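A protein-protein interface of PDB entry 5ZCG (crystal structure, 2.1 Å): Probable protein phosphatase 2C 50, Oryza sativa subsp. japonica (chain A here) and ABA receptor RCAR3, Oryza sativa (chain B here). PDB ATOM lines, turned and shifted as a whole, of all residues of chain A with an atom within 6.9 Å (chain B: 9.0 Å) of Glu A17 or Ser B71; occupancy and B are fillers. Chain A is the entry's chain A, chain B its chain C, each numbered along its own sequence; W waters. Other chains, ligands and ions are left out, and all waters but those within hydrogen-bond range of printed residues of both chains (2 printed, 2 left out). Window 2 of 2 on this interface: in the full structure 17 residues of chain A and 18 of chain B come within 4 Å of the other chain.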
ATOM      1  N   ARG A  10       8.345   6.380  23.256  1.00  0.00           N
ATOM      2  CA  ARG A  10       8.717   5.755  21.996  1.00  0.00           C
ATOM      3  C   ARG A  10      10.211   5.463  21.938  1.00  0.00           C
ATOM      4  O   ARG A  10      10.637   4.605  21.156  1.00  0.00           O
ATOM      5  CB  ARG A  10       8.289   6.649  20.832  1.00  0.00           C
ATOM      6  CG  ARG A  10       9.213   7.827  20.577  1.00  0.00           C
ATOM      7  CD  ARG A  10       8.601   8.802  19.581  1.00  0.00           C
ATOM      8  NE  ARG A  10       9.373  10.037  19.487  1.00  0.00           N
ATOM      9  CZ  ARG A  10      10.548  10.140  18.872  1.00  0.00           C
ATOM     10  NH1 ARG A  10      11.092   9.077  18.293  1.00  0.00           N
ATOM     11  NH2 ARG A  10      11.181  11.304  18.836  1.00  0.00           N
ATOM     12  N   GLU A  15       7.969   5.922  15.790  1.00  0.00           N
ATOM     13  CA  GLU A  15       6.634   6.145  16.327  1.00  0.00           C
ATOM     14  C   GLU A  15       6.372   5.261  17.541  1.00  0.00           C
ATOM     15  O   GLU A  15       6.993   4.211  17.732  1.00  0.00           O
ATOM     16  CB  GLU A  15       5.564   5.919  15.253  1.00  0.00           C
ATOM     17  CG  GLU A  15       5.372   7.142  14.366  1.00  0.00           C
ATOM     18  CD  GLU A  15       5.528   6.839  12.891  1.00  0.00           C
ATOM     19  OE1 GLU A  15       5.852   7.775  12.131  1.00  0.00           O
ATOM     20  OE2 GLU A  15       5.307   5.677  12.487  1.00  0.00           O
ATOM     21  N   MET A  16       5.415   5.702  18.353  1.00  0.00           N
ATOM     22  CA  MET A  16       5.025   5.004  19.569  1.00  0.00           C
ATOM     23  C   MET A  16       3.913   4.004  19.267  1.00  0.00           C
ATOM     24  O   MET A  16       2.844   4.384  18.774  1.00  0.00           O
ATOM     25  CB  MET A  16       4.556   5.999  20.628  1.00  0.00           C
ATOM     26  CG  MET A  16       4.074   5.346  21.900  1.00  0.00           C
ATOM     27  SD  MET A  16       5.351   4.314  22.635  1.00  0.00           S
ATOM     28  CE  MET A  16       5.043   4.603  24.380  1.00  0.00           C
ATOM     29  N   GLU A  17       4.158   2.731  19.584  1.00  0.00           N
ATOM     30  CA  GLU A  17       3.161   1.684  19.410  1.00  0.00           C
ATOM     31  C   GLU A  17       2.903   0.895  20.683  1.00  0.00           C
ATOM     32  O   GLU A  17       2.133  -0.073  20.648  1.00  0.00           O
ATOM     33  CB  GLU A  17       3.578   0.730  18.284  1.00  0.00           C
ATOM     34  CG  GLU A  17       3.770   1.441  16.950  1.00  0.00           C
ATOM     35  CD  GLU A  17       4.270   0.518  15.860  1.00  0.00           C
ATOM     36  OE1 GLU A  17       4.117   0.872  14.672  1.00  0.00           O
ATOM     37  OE2 GLU A  17       4.818  -0.556  16.188  1.00  0.00           O
ATOM     38  N   ASP A  18       3.538   1.262  21.790  1.00  0.00           N
ATOM     39  CA  ASP A  18       3.161   0.751  23.096  1.00  0.00           C
ATOM     40  C   ASP A  18       1.924   1.493  23.585  1.00  0.00           C
ATOM     41  O   ASP A  18       1.739   2.683  23.307  1.00  0.00           O
ATOM     42  CB  ASP A  18       4.294   0.957  24.105  1.00  0.00           C
ATOM     43  CG  ASP A  18       5.316  -0.168  24.108  1.00  0.00           C
ATOM     44  OD1 ASP A  18       5.325  -0.997  23.175  1.00  0.00           O
ATOM     45  OD2 ASP A  18       6.135  -0.200  25.053  1.00  0.00           O
ATOM     46  N   ALA A  19       1.068   0.776  24.314  1.00  0.00           N
ATOM     47  CA  ALA A  19      -0.066   1.369  25.005  1.00  0.00           C
ATOM     48  C   ALA A  19      -0.135   0.782  26.406  1.00  0.00           C
ATOM     49  O   ALA A  19       0.437  -0.276  26.690  1.00  0.00           O
ATOM     50  CB  ALA A  19      -1.386   1.130  24.259  1.00  0.00           C
ATOM     51  N   PHE A  60       0.354  -3.184  26.607  1.00  0.00           N
ATOM     52  CA  PHE A  60       0.011  -3.723  25.296  1.00  0.00           C
ATOM     53  C   PHE A  60       1.060  -3.241  24.304  1.00  0.00           C
ATOM     54  O   PHE A  60       1.095  -2.059  23.954  1.00  0.00           O
ATOM     55  CB  PHE A  60      -1.391  -3.281  24.880  1.00  0.00           C
ATOM     56  CG  PHE A  60      -2.382  -3.301  26.012  1.00  0.00           C
ATOM     57  CD1 PHE A  60      -2.986  -4.485  26.398  1.00  0.00           C
ATOM     58  CD2 PHE A  60      -2.678  -2.143  26.713  1.00  0.00           C
ATOM     59  CE1 PHE A  60      -3.883  -4.515  27.447  1.00  0.00           C
ATOM     60  CE2 PHE A  60      -3.572  -2.164  27.764  1.00  0.00           C
ATOM     61  CZ  PHE A  60      -4.178  -3.353  28.131  1.00  0.00           C
ATOM     62  N   ASP A  61       1.902  -4.152  23.847  1.00  0.00           N
ATOM     63  CA  ASP A  61       3.010  -3.831  22.953  1.00  0.00           C
ATOM     64  C   ASP A  61       2.535  -4.109  21.530  1.00  0.00           C
ATOM     65  O   ASP A  61       2.456  -5.262  21.103  1.00  0.00           O
ATOM     66  CB  ASP A  61       4.235  -4.650  23.350  1.00  0.00           C
ATOM     67  CG  ASP A  61       5.448  -4.387  22.479  1.00  0.00           C
ATOM     68  OD1 ASP A  61       5.343  -3.697  21.441  1.00  0.00           O
ATOM     69  OD2 ASP A  61       6.525  -4.892  22.853  1.00  0.00           O
ATOM     70  N   GLY A  62       2.214  -3.044  20.797  1.00  0.00           N
ATOM     71  CA  GLY A  62       1.752  -3.201  19.433  1.00  0.00           C
ATOM     72  C   GLY A  62       2.897  -3.360  18.444  1.00  0.00           C
ATOM     73  O   GLY A  62       4.004  -2.869  18.652  1.00  0.00           O
ATOM     74  N   HIS A  63       2.623  -4.108  17.375  1.00  0.00           N
ATOM     75  CA  HIS A  63       3.506  -4.236  16.223  1.00  0.00           C
ATOM     76  C   HIS A  63       2.664  -4.103  14.959  1.00  0.00           C
ATOM     77  O   HIS A  63       1.456  -4.357  14.966  1.00  0.00           O
ATOM     78  CB  HIS A  63       4.276  -5.567  16.221  1.00  0.00           C
ATOM     79  CG  HIS A  63       3.402  -6.771  16.377  1.00  0.00           C
ATOM     80  ND1 HIS A  63       3.183  -7.378  17.596  1.00  0.00           N
ATOM     81  CD2 HIS A  63       2.679  -7.472  15.472  1.00  0.00           C
ATOM     82  CE1 HIS A  63       2.367  -8.403  17.434  1.00  0.00           C
ATOM     83  NE2 HIS A  63       2.046  -8.483  16.155  1.00  0.00           N
ATOM     84  N   GLY A  64       3.311  -3.693  13.870  1.00  0.00           N
ATOM     85  CA  GLY A  64       2.617  -3.362  12.639  1.00  0.00           C
ATOM     86  C   GLY A  64       1.850  -2.062  12.678  1.00  0.00           C
ATOM     87  O   GLY A  64       1.278  -1.660  11.658  1.00  0.00           O
ATOM     88  N   GLY A  65       1.850  -1.380  13.806  1.00  0.00           N
ATOM     89  CA  GLY A  65       1.024  -0.208  14.020  1.00  0.00           C
ATOM     90  C   GLY A  65       0.641  -0.121  15.481  1.00  0.00           C
ATOM     91  O   GLY A  65       0.922  -1.016  16.277  1.00  0.00           O
ATOM     92  N   ALA A  66      -0.023   0.979  15.829  1.00  0.00           N
ATOM     93  CA  ALA A  66      -0.465   1.205  17.199  1.00  0.00           C
ATOM     94  C   ALA A  66      -1.936   0.857  17.424  1.00  0.00           C
ATOM     95  O   ALA A  66      -2.398   0.898  18.569  1.00  0.00           O
ATOM     96  CB  ALA A  66      -0.225   2.662  17.599  1.00  0.00           C
ATOM     97  N   GLU A  67      -2.672   0.467  16.379  1.00  0.00           N
ATOM     98  CA  GLU A  67      -4.128   0.456  16.485  1.00  0.00           C
ATOM     99  C   GLU A  67      -4.631  -0.683  17.363  1.00  0.00           C
ATOM    100  O   GLU A  67      -5.601  -0.509  18.109  1.00  0.00           O
ATOM    101  CB  GLU A  67      -4.755   0.358  15.092  1.00  0.00           C
ATOM    102  CG  GLU A  67      -4.483   1.547  14.179  1.00  0.00           C
ATOM    103  CD  GLU A  67      -3.150   1.439  13.460  1.00  0.00           C
ATOM    104  OE1 GLU A  67      -2.609   2.488  13.055  1.00  0.00           O
ATOM    105  OE2 GLU A  67      -2.641   0.309  13.303  1.00  0.00           O
ATOM    106  N   VAL A  68      -3.983  -1.847  17.313  1.00  0.00           N
ATOM    107  CA  VAL A  68      -4.443  -2.961  18.139  1.00  0.00           C
ATOM    108  C   VAL A  68      -4.040  -2.761  19.597  1.00  0.00           C
ATOM    109  O   VAL A  68      -4.810  -3.072  20.511  1.00  0.00           O
ATOM    110  CB  VAL A  68      -3.936  -4.301  17.575  1.00  0.00           C
ATOM    111  CG1 VAL A  68      -4.326  -5.462  18.488  1.00  0.00           C
ATOM    112  CG2 VAL A  68      -4.490  -4.525  16.176  1.00  0.00           C
ATOM    113  N   ALA A  69      -2.851  -2.211  19.845  1.00  0.00           N
ATOM    114  CA  ALA A  69      -2.471  -1.894  21.221  1.00  0.00           C
ATOM    115  C   ALA A  69      -3.424  -0.874  21.842  1.00  0.00           C
ATOM    116  O   ALA A  69      -3.827  -1.012  23.005  1.00  0.00           O
ATOM    117  CB  ALA A  69      -1.029  -1.384  21.262  1.00  0.00           C
ATOM    118  N   ASN A  70      -3.803   0.153  21.076  1.00  0.00           N
ATOM    119  CA  ASN A  70      -4.742   1.153  21.578  1.00  0.00           C
ATOM    120  C   ASN A  70      -6.128   0.560  21.776  1.00  0.00           C
ATOM    121  O   ASN A  70      -6.817   0.880  22.759  1.00  0.00           O
ATOM    122  CB  ASN A  70      -4.810   2.339  20.617  1.00  0.00           C
ATOM    123  CG  ASN A  70      -3.553   3.181  20.645  1.00  0.00           C
ATOM    124  OD1 ASN A  70      -2.760   3.094  21.580  1.00  0.00           O
ATOM    125  ND2 ASN A  70      -3.363   3.996  19.617  1.00  0.00           N
ATOM    126  N   ASN A 141      -1.978  -7.660   9.439  1.00  0.00           N
ATOM    127  CA  ASN A 141      -0.647  -7.832  10.010  1.00  0.00           C
ATOM    128  C   ASN A 141      -0.372  -6.850  11.144  1.00  0.00           C
ATOM    129  O   ASN A 141       0.787  -6.516  11.410  1.00  0.00           O
ATOM    130  CB  ASN A 141       0.424  -7.710   8.927  1.00  0.00           C
ATOM    131  CG  ASN A 141       0.397  -6.369   8.224  1.00  0.00           C
ATOM    132  OD1 ASN A 141      -0.513  -5.567   8.425  1.00  0.00           O
ATOM    133  ND2 ASN A 141       1.393  -6.125   7.379  1.00  0.00           N
ATOM    134  N   GLY A 143      -0.874  -6.222  15.279  1.00  0.00           N
ATOM    135  CA  GLY A 143      -1.129  -6.992  16.477  1.00  0.00           C
ATOM    136  C   GLY A 143      -0.641  -6.288  17.725  1.00  0.00           C
ATOM    137  O   GLY A 143      -0.163  -5.150  17.685  1.00  0.00           O
ATOM    138  N   SER A 144      -0.759  -6.991  18.848  1.00  0.00           N
ATOM    139  CA  SER A 144      -0.270  -6.444  20.101  1.00  0.00           C
ATOM    140  C   SER A 144      -0.111  -7.565  21.114  1.00  0.00           C
ATOM    141  O   SER A 144      -0.818  -8.574  21.060  1.00  0.00           O
ATOM    142  CB  SER A 144      -1.214  -5.369  20.649  1.00  0.00           C
ATOM    143  OG  SER A 144      -0.814  -4.967  21.948  1.00  0.00           O
ATOM    144  N   LEU A 211       7.364 -13.517  12.863  1.00  0.00           N
ATOM    145  CA  LEU A 211       6.947 -12.879  14.105  1.00  0.00           C
ATOM    146  C   LEU A 211       7.644 -13.543  15.280  1.00  0.00           C
ATOM    147  O   LEU A 211       7.613 -14.769  15.416  1.00  0.00           O
ATOM    148  CB  LEU A 211       5.424 -12.973  14.273  1.00  0.00           C
ATOM    149  CG  LEU A 211       4.747 -12.137  15.360  1.00  0.00           C
ATOM    150  CD1 LEU A 211       4.668 -10.682  14.926  1.00  0.00           C
ATOM    151  CD2 LEU A 211       3.363 -12.674  15.653  1.00  0.00           C
ATOM    152  N   ASP A 311      13.707  -0.093  21.453  1.00  0.00           N
ATOM    153  CA  ASP A 311      12.268  -0.173  21.259  1.00  0.00           C
ATOM    154  C   ASP A 311      11.513   0.893  22.047  1.00  0.00           C
ATOM    155  O   ASP A 311      12.071   1.639  22.861  1.00  0.00           O
ATOM    156  CB  ASP A 311      11.776  -1.559  21.676  1.00  0.00           C
ATOM    157  CG  ASP A 311      10.518  -1.976  20.966  1.00  0.00           C
ATOM    158  OD1 ASP A 311       9.853  -1.125  20.340  1.00  0.00           O
ATOM    159  OD2 ASP A 311      10.185  -3.170  21.050  1.00  0.00           O
ATOM    160  N   ASN A 312      10.206   0.954  21.792  1.00  0.00           N
ATOM    161  CA  ASN A 312       9.311   1.619  22.723  1.00  0.00           C
ATOM    162  C   ASN A 312       9.474   0.973  24.092  1.00  0.00           C
ATOM    163  O   ASN A 312       9.728  -0.229  24.208  1.00  0.00           O
ATOM    164  CB  ASN A 312       7.851   1.495  22.274  1.00  0.00           C
ATOM    165  CG  ASN A 312       7.615   1.973  20.849  1.00  0.00           C
ATOM    166  OD1 ASN A 312       6.650   1.559  20.202  1.00  0.00           O
ATOM    167  ND2 ASN A 312       8.479   2.856  20.360  1.00  0.00           N
ATOM    168  N   THR A 314       7.569   0.816  27.925  1.00  0.00           N
ATOM    169  CA  THR A 314       6.422   1.132  28.764  1.00  0.00           C
ATOM    170  C   THR A 314       6.546   0.336  30.050  1.00  0.00           C
ATOM    171  O   THR A 314       6.766  -0.876  30.013  1.00  0.00           O
ATOM    172  CB  THR A 314       5.102   0.824  28.055  1.00  0.00           C
ATOM    173  OG1 THR A 314       4.933   1.757  26.983  1.00  0.00           O
ATOM    174  CG2 THR A 314       3.925   0.962  29.016  1.00  0.00           C
ATOM    175  N   PRO B  48       1.537  -4.991   2.207  1.00  0.00           N
ATOM    176  CA  PRO B  48       1.011  -4.672   3.544  1.00  0.00           C
ATOM    177  C   PRO B  48       2.072  -4.445   4.609  1.00  0.00           C
ATOM    178  O   PRO B  48       1.725  -3.989   5.708  1.00  0.00           O
ATOM    179  CB  PRO B  48       0.153  -5.901   3.882  1.00  0.00           C
ATOM    180  CG  PRO B  48       0.757  -7.015   3.094  1.00  0.00           C
ATOM    181  CD  PRO B  48       1.285  -6.393   1.823  1.00  0.00           C
ATOM    182  N   PHE B  49       3.341  -4.738   4.335  1.00  0.00           N
ATOM    183  CA  PHE B  49       4.391  -4.529   5.323  1.00  0.00           C
ATOM    184  C   PHE B  49       5.147  -3.221   5.137  1.00  0.00           C
ATOM    185  O   PHE B  49       5.944  -2.862   6.010  1.00  0.00           O
ATOM    186  CB  PHE B  49       5.382  -5.696   5.302  1.00  0.00           C
ATOM    187  CG  PHE B  49       4.773  -7.009   5.700  1.00  0.00           C
ATOM    188  CD1 PHE B  49       4.450  -7.262   7.023  1.00  0.00           C
ATOM    189  CD2 PHE B  49       4.522  -7.990   4.753  1.00  0.00           C
ATOM    190  CE1 PHE B  49       3.884  -8.471   7.399  1.00  0.00           C
ATOM    191  CE2 PHE B  49       3.954  -9.203   5.121  1.00  0.00           C
ATOM    192  CZ  PHE B  49       3.636  -9.442   6.446  1.00  0.00           C
ATOM    193  N   VAL B  50       4.925  -2.506   4.037  1.00  0.00           N
ATOM    194  CA  VAL B  50       5.638  -1.259   3.771  1.00  0.00           C
ATOM    195  C   VAL B  50       4.970  -0.122   4.537  1.00  0.00           C
ATOM    196  O   VAL B  50       3.767   0.114   4.391  1.00  0.00           O
ATOM    197  CB  VAL B  50       5.684  -0.956   2.265  1.00  0.00           C
ATOM    198  CG1 VAL B  50       6.370   0.385   2.010  1.00  0.00           C
ATOM    199  CG2 VAL B  50       6.390  -2.081   1.508  1.00  0.00           C
ATOM    200  N   SER B  51       5.750   0.582   5.356  1.00  0.00           N
ATOM    201  CA  SER B  51       5.296   1.770   6.065  1.00  0.00           C
ATOM    202  C   SER B  51       5.666   3.064   5.355  1.00  0.00           C
ATOM    203  O   SER B  51       4.899   4.031   5.411  1.00  0.00           O
ATOM    204  CB  SER B  51       5.874   1.796   7.482  1.00  0.00           C
ATOM    205  OG  SER B  51       7.283   1.918   7.444  1.00  0.00           O
ATOM    206  N   ARG B  52       6.824   3.109   4.701  1.00  0.00           N
ATOM    207  CA  ARG B  52       7.256   4.289   3.970  1.00  0.00           C
ATOM    208  C   ARG B  52       8.065   3.848   2.763  1.00  0.00           C
ATOM    209  O   ARG B  52       8.734   2.814   2.795  1.00  0.00           O
ATOM    210  CB  ARG B  52       8.127   5.219   4.835  1.00  0.00           C
ATOM    211  CG  ARG B  52       7.447   5.852   6.034  1.00  0.00           C
ATOM    212  CD  ARG B  52       8.481   6.374   7.035  1.00  0.00           C
ATOM    213  NE  ARG B  52       9.083   5.302   7.827  1.00  0.00           N
ATOM    214  CZ  ARG B  52      10.155   5.450   8.604  1.00  0.00           C
ATOM    215  NH1 ARG B  52      10.754   6.631   8.698  1.00  0.00           N
ATOM    216  NH2 ARG B  52      10.630   4.416   9.287  1.00  0.00           N
ATOM    217  N   ASN B  68      10.906   1.500   4.185  1.00  0.00           N
ATOM    218  CA  ASN B  68      10.864   1.151   5.593  1.00  0.00           C
ATOM    219  C   ASN B  68       9.666   0.241   5.796  1.00  0.00           C
ATOM    220  O   ASN B  68       8.597   0.484   5.231  1.00  0.00           O
ATOM    221  CB  ASN B  68      10.747   2.394   6.477  1.00  0.00           C
ATOM    222  CG  ASN B  68      11.988   3.265   6.431  1.00  0.00           C
ATOM    223  OD1 ASN B  68      12.097   4.163   5.597  1.00  0.00           O
ATOM    224  ND2 ASN B  68      12.930   3.004   7.328  1.00  0.00           N
ATOM    225  N   VAL B  69       9.846  -0.822   6.564  1.00  0.00           N
ATOM    226  CA  VAL B  69       8.768  -1.752   6.811  1.00  0.00           C
ATOM    227  C   VAL B  69       8.240  -1.522   8.221  1.00  0.00           C
ATOM    228  O   VAL B  69       8.865  -0.858   9.054  1.00  0.00           O
ATOM    229  CB  VAL B  69       9.192  -3.226   6.599  1.00  0.00           C
ATOM    230  CG1 VAL B  69       9.504  -3.481   5.125  1.00  0.00           C
ATOM    231  CG2 VAL B  69      10.370  -3.583   7.480  1.00  0.00           C
ATOM    232  N   LYS B  70       7.054  -2.059   8.483  1.00  0.00           N
ATOM    233  CA  LYS B  70       6.429  -1.891   9.783  1.00  0.00           C
ATOM    234  C   LYS B  70       7.131  -2.755  10.829  1.00  0.00           C
ATOM    235  O   LYS B  70       7.900  -3.667  10.509  1.00  0.00           O
ATOM    236  CB  LYS B  70       4.942  -2.233   9.701  1.00  0.00           C
ATOM    237  CG  LYS B  70       4.189  -1.366   8.707  1.00  0.00           C
ATOM    238  CD  LYS B  70       2.767  -1.850   8.493  1.00  0.00           C
ATOM    239  CE  LYS B  70       2.041  -0.951   7.505  1.00  0.00           C
ATOM    240  NZ  LYS B  70       0.676  -1.457   7.191  1.00  0.00           N
ATOM    241  N   SER B  71       6.865  -2.443  12.096  1.00  0.00           N
ATOM    242  CA  SER B  71       7.498  -3.128  13.216  1.00  0.00           C
ATOM    243  C   SER B  71       7.025  -4.581  13.313  1.00  0.00           C
ATOM    244  O   SER B  71       6.039  -4.995  12.691  1.00  0.00           O
ATOM    245  CB  SER B  71       7.193  -2.397  14.522  1.00  0.00           C
ATOM    246  OG  SER B  71       5.808  -2.107  14.609  1.00  0.00           O
ATOM    247  N   GLY B  72       7.741  -5.356  14.132  1.00  0.00           N
ATOM    248  CA  GLY B  72       7.455  -6.764  14.326  1.00  0.00           C
ATOM    249  C   GLY B  72       8.164  -7.716  13.380  1.00  0.00           C
ATOM    250  O   GLY B  72       8.137  -8.931  13.618  1.00  0.00           O
ATOM    251  N   LEU B  73       8.813  -7.206  12.322  1.00  0.00           N
ATOM    252  CA  LEU B  73       9.457  -7.985  11.272  1.00  0.00           C
ATOM    253  C   LEU B  73      10.928  -8.241  11.594  1.00  0.00           C
ATOM    254  O   LEU B  73      11.507  -7.592  12.468  1.00  0.00           O
ATOM    255  CB  LEU B  73       9.332  -7.248   9.938  1.00  0.00           C
ATOM    256  CG  LEU B  73       7.925  -7.198   9.343  1.00  0.00           C
ATOM    257  CD1 LEU B  73       7.888  -6.295   8.123  1.00  0.00           C
ATOM    258  CD2 LEU B  73       7.446  -8.595   8.994  1.00  0.00           C
ATOM    259  N   PRO B  74      11.565  -9.199  10.907  1.00  0.00           N
ATOM    260  CA  PRO B  74      12.997  -9.448  11.148  1.00  0.00           C
ATOM    261  C   PRO B  74      13.907  -8.305  10.732  1.00  0.00           C
ATOM    262  O   PRO B  74      15.082  -8.310  11.116  1.00  0.00           O
ATOM    263  CB  PRO B  74      13.284 -10.704  10.310  1.00  0.00           C
ATOM    264  CG  PRO B  74      11.966 -11.328  10.074  1.00  0.00           C
ATOM    265  CD  PRO B  74      10.985 -10.207  10.004  1.00  0.00           C
ATOM    266  N   ALA B  75      13.411  -7.335   9.965  1.00  0.00           N
ATOM    267  CA  ALA B  75      14.214  -6.223   9.477  1.00  0.00           C
ATOM    268  C   ALA B  75      13.381  -4.950   9.518  1.00  0.00           C
ATOM    269  O   ALA B  75      12.177  -4.976   9.794  1.00  0.00           O
ATOM    270  CB  ALA B  75      14.722  -6.478   8.054  1.00  0.00           C
ATOM    271  N   THR B  76      14.033  -3.824   9.225  1.00  0.00           N
ATOM    272  CA  THR B  76      13.365  -2.531   9.235  1.00  0.00           C
ATOM    273  C   THR B  76      13.383  -1.801   7.900  1.00  0.00           C
ATOM    274  O   THR B  76      12.470  -1.017   7.636  1.00  0.00           O
ATOM    275  CB  THR B  76      13.987  -1.611  10.300  1.00  0.00           C
ATOM    276  OG1 THR B  76      15.365  -1.371   9.984  1.00  0.00           O
ATOM    277  CG2 THR B  76      13.883  -2.246  11.690  1.00  0.00           C
HETATM  278  O   HOH W   1      -0.955  -3.298   6.564  1.00  0.00           O
HETATM  279  O   HOH W   2       4.890  -0.373  12.581  1.00  0.00           O
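The side-chain carboxylate (OE2) of Glu A17 lies within hydrogen-bond range of the side-chain hydroxyl (OG) of Ser B71 (2.4 Å).
N of Gly A64 sits at hydrogen-bond distance from OG of Ser B71, at 3.0 Å.
The side-chain amide nitrogen (ND2) of Asn A141 sits at hydrogen-bond distance from the backbone carbonyl oxygen (O) of Pro B48 (2.7 Å).
The backbone carbonyl oxygen (O) of Glu A17 lies within hydrogen-bond range of the backbone NH (N) of Gly A62 (3.0 Å).
N of Gly A65 lies within hydrogen-bond range of OE1 of Glu A17.
N of Glu A17 sits at hydrogen-bond distance from OD1 of Asn A312 (2.8 Å).
N of His A63 lies within hydrogen-bond range of O of Gly A143 (3.0 Å).
The backbone carbonyl oxygen of Pro B48 sits at hydrogen-bond distance from the side-chain amino group of Lys B70 (3.1 Å).
The backbone NH of Lys B70 lies within hydrogen-bond range of the backbone carbonyl oxygen of Phe B49 (2.8 Å).
OG of Ser B71 touches CA of His A63, 3.5 Å away.
CA of Gly B72 touches CB of His A63, at 3.9 Å.
Gly A64 touches Lys B70 (O to CD, 3.5 Å).
CD1 of Phe B49 touches ND2 of Asn A141, 3.3 Å away.
Of chain B, only Ser B71 comes within 4 Å of Glu A17.
Ser B71 touches just these residues of chain A: Glu A17, His A63 and Gly A64.
No residue of chain B comes within 4 Å of Gly A62.
Gly A64 touches just these residues of chain B: Lys B70 (3.5 Å) and Ser B71 (3.0 Å).
Of the printed residues of chain A, Lys B70 touches Gly A64.
Printed residues of chain A within 4 Å of Gly B72: His A63 (3.9 Å).
Val A68 touches none of the printed residues of chain B.
Ser A144 touches none of the printed residues of chain B.
The nearest residue of chain A that does not touch Ser B71 is Gly A65 (4.1 Å).
The nearest printed residue of chain A that does not touch Pro B48 is Gly A64 (6.4 Å).
Of the 24 printed residues of chain A, 4 touch a printed residue of chain B.
Hydrophobic or aromatic side chains of chain A that line the printed part of chain B: His A63.
Among the printed residues, 7 pairs touch across the chains.
Among the printed residues, no Asp or Glu carboxylate lies within 4 Å of a Lys or Arg side-chain nitrogen of the other chain.
Water W1 lies within hydrogen-bond range of NZ of Lys B70, O of Pro B48 and OD1 of Asn A141.
Water W2 lies within hydrogen-bond range of OE1 of Glu A17 (2.6 Å), OG of Ser B71 (2.8 Å) and N of Gly A65 (3.4 Å).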
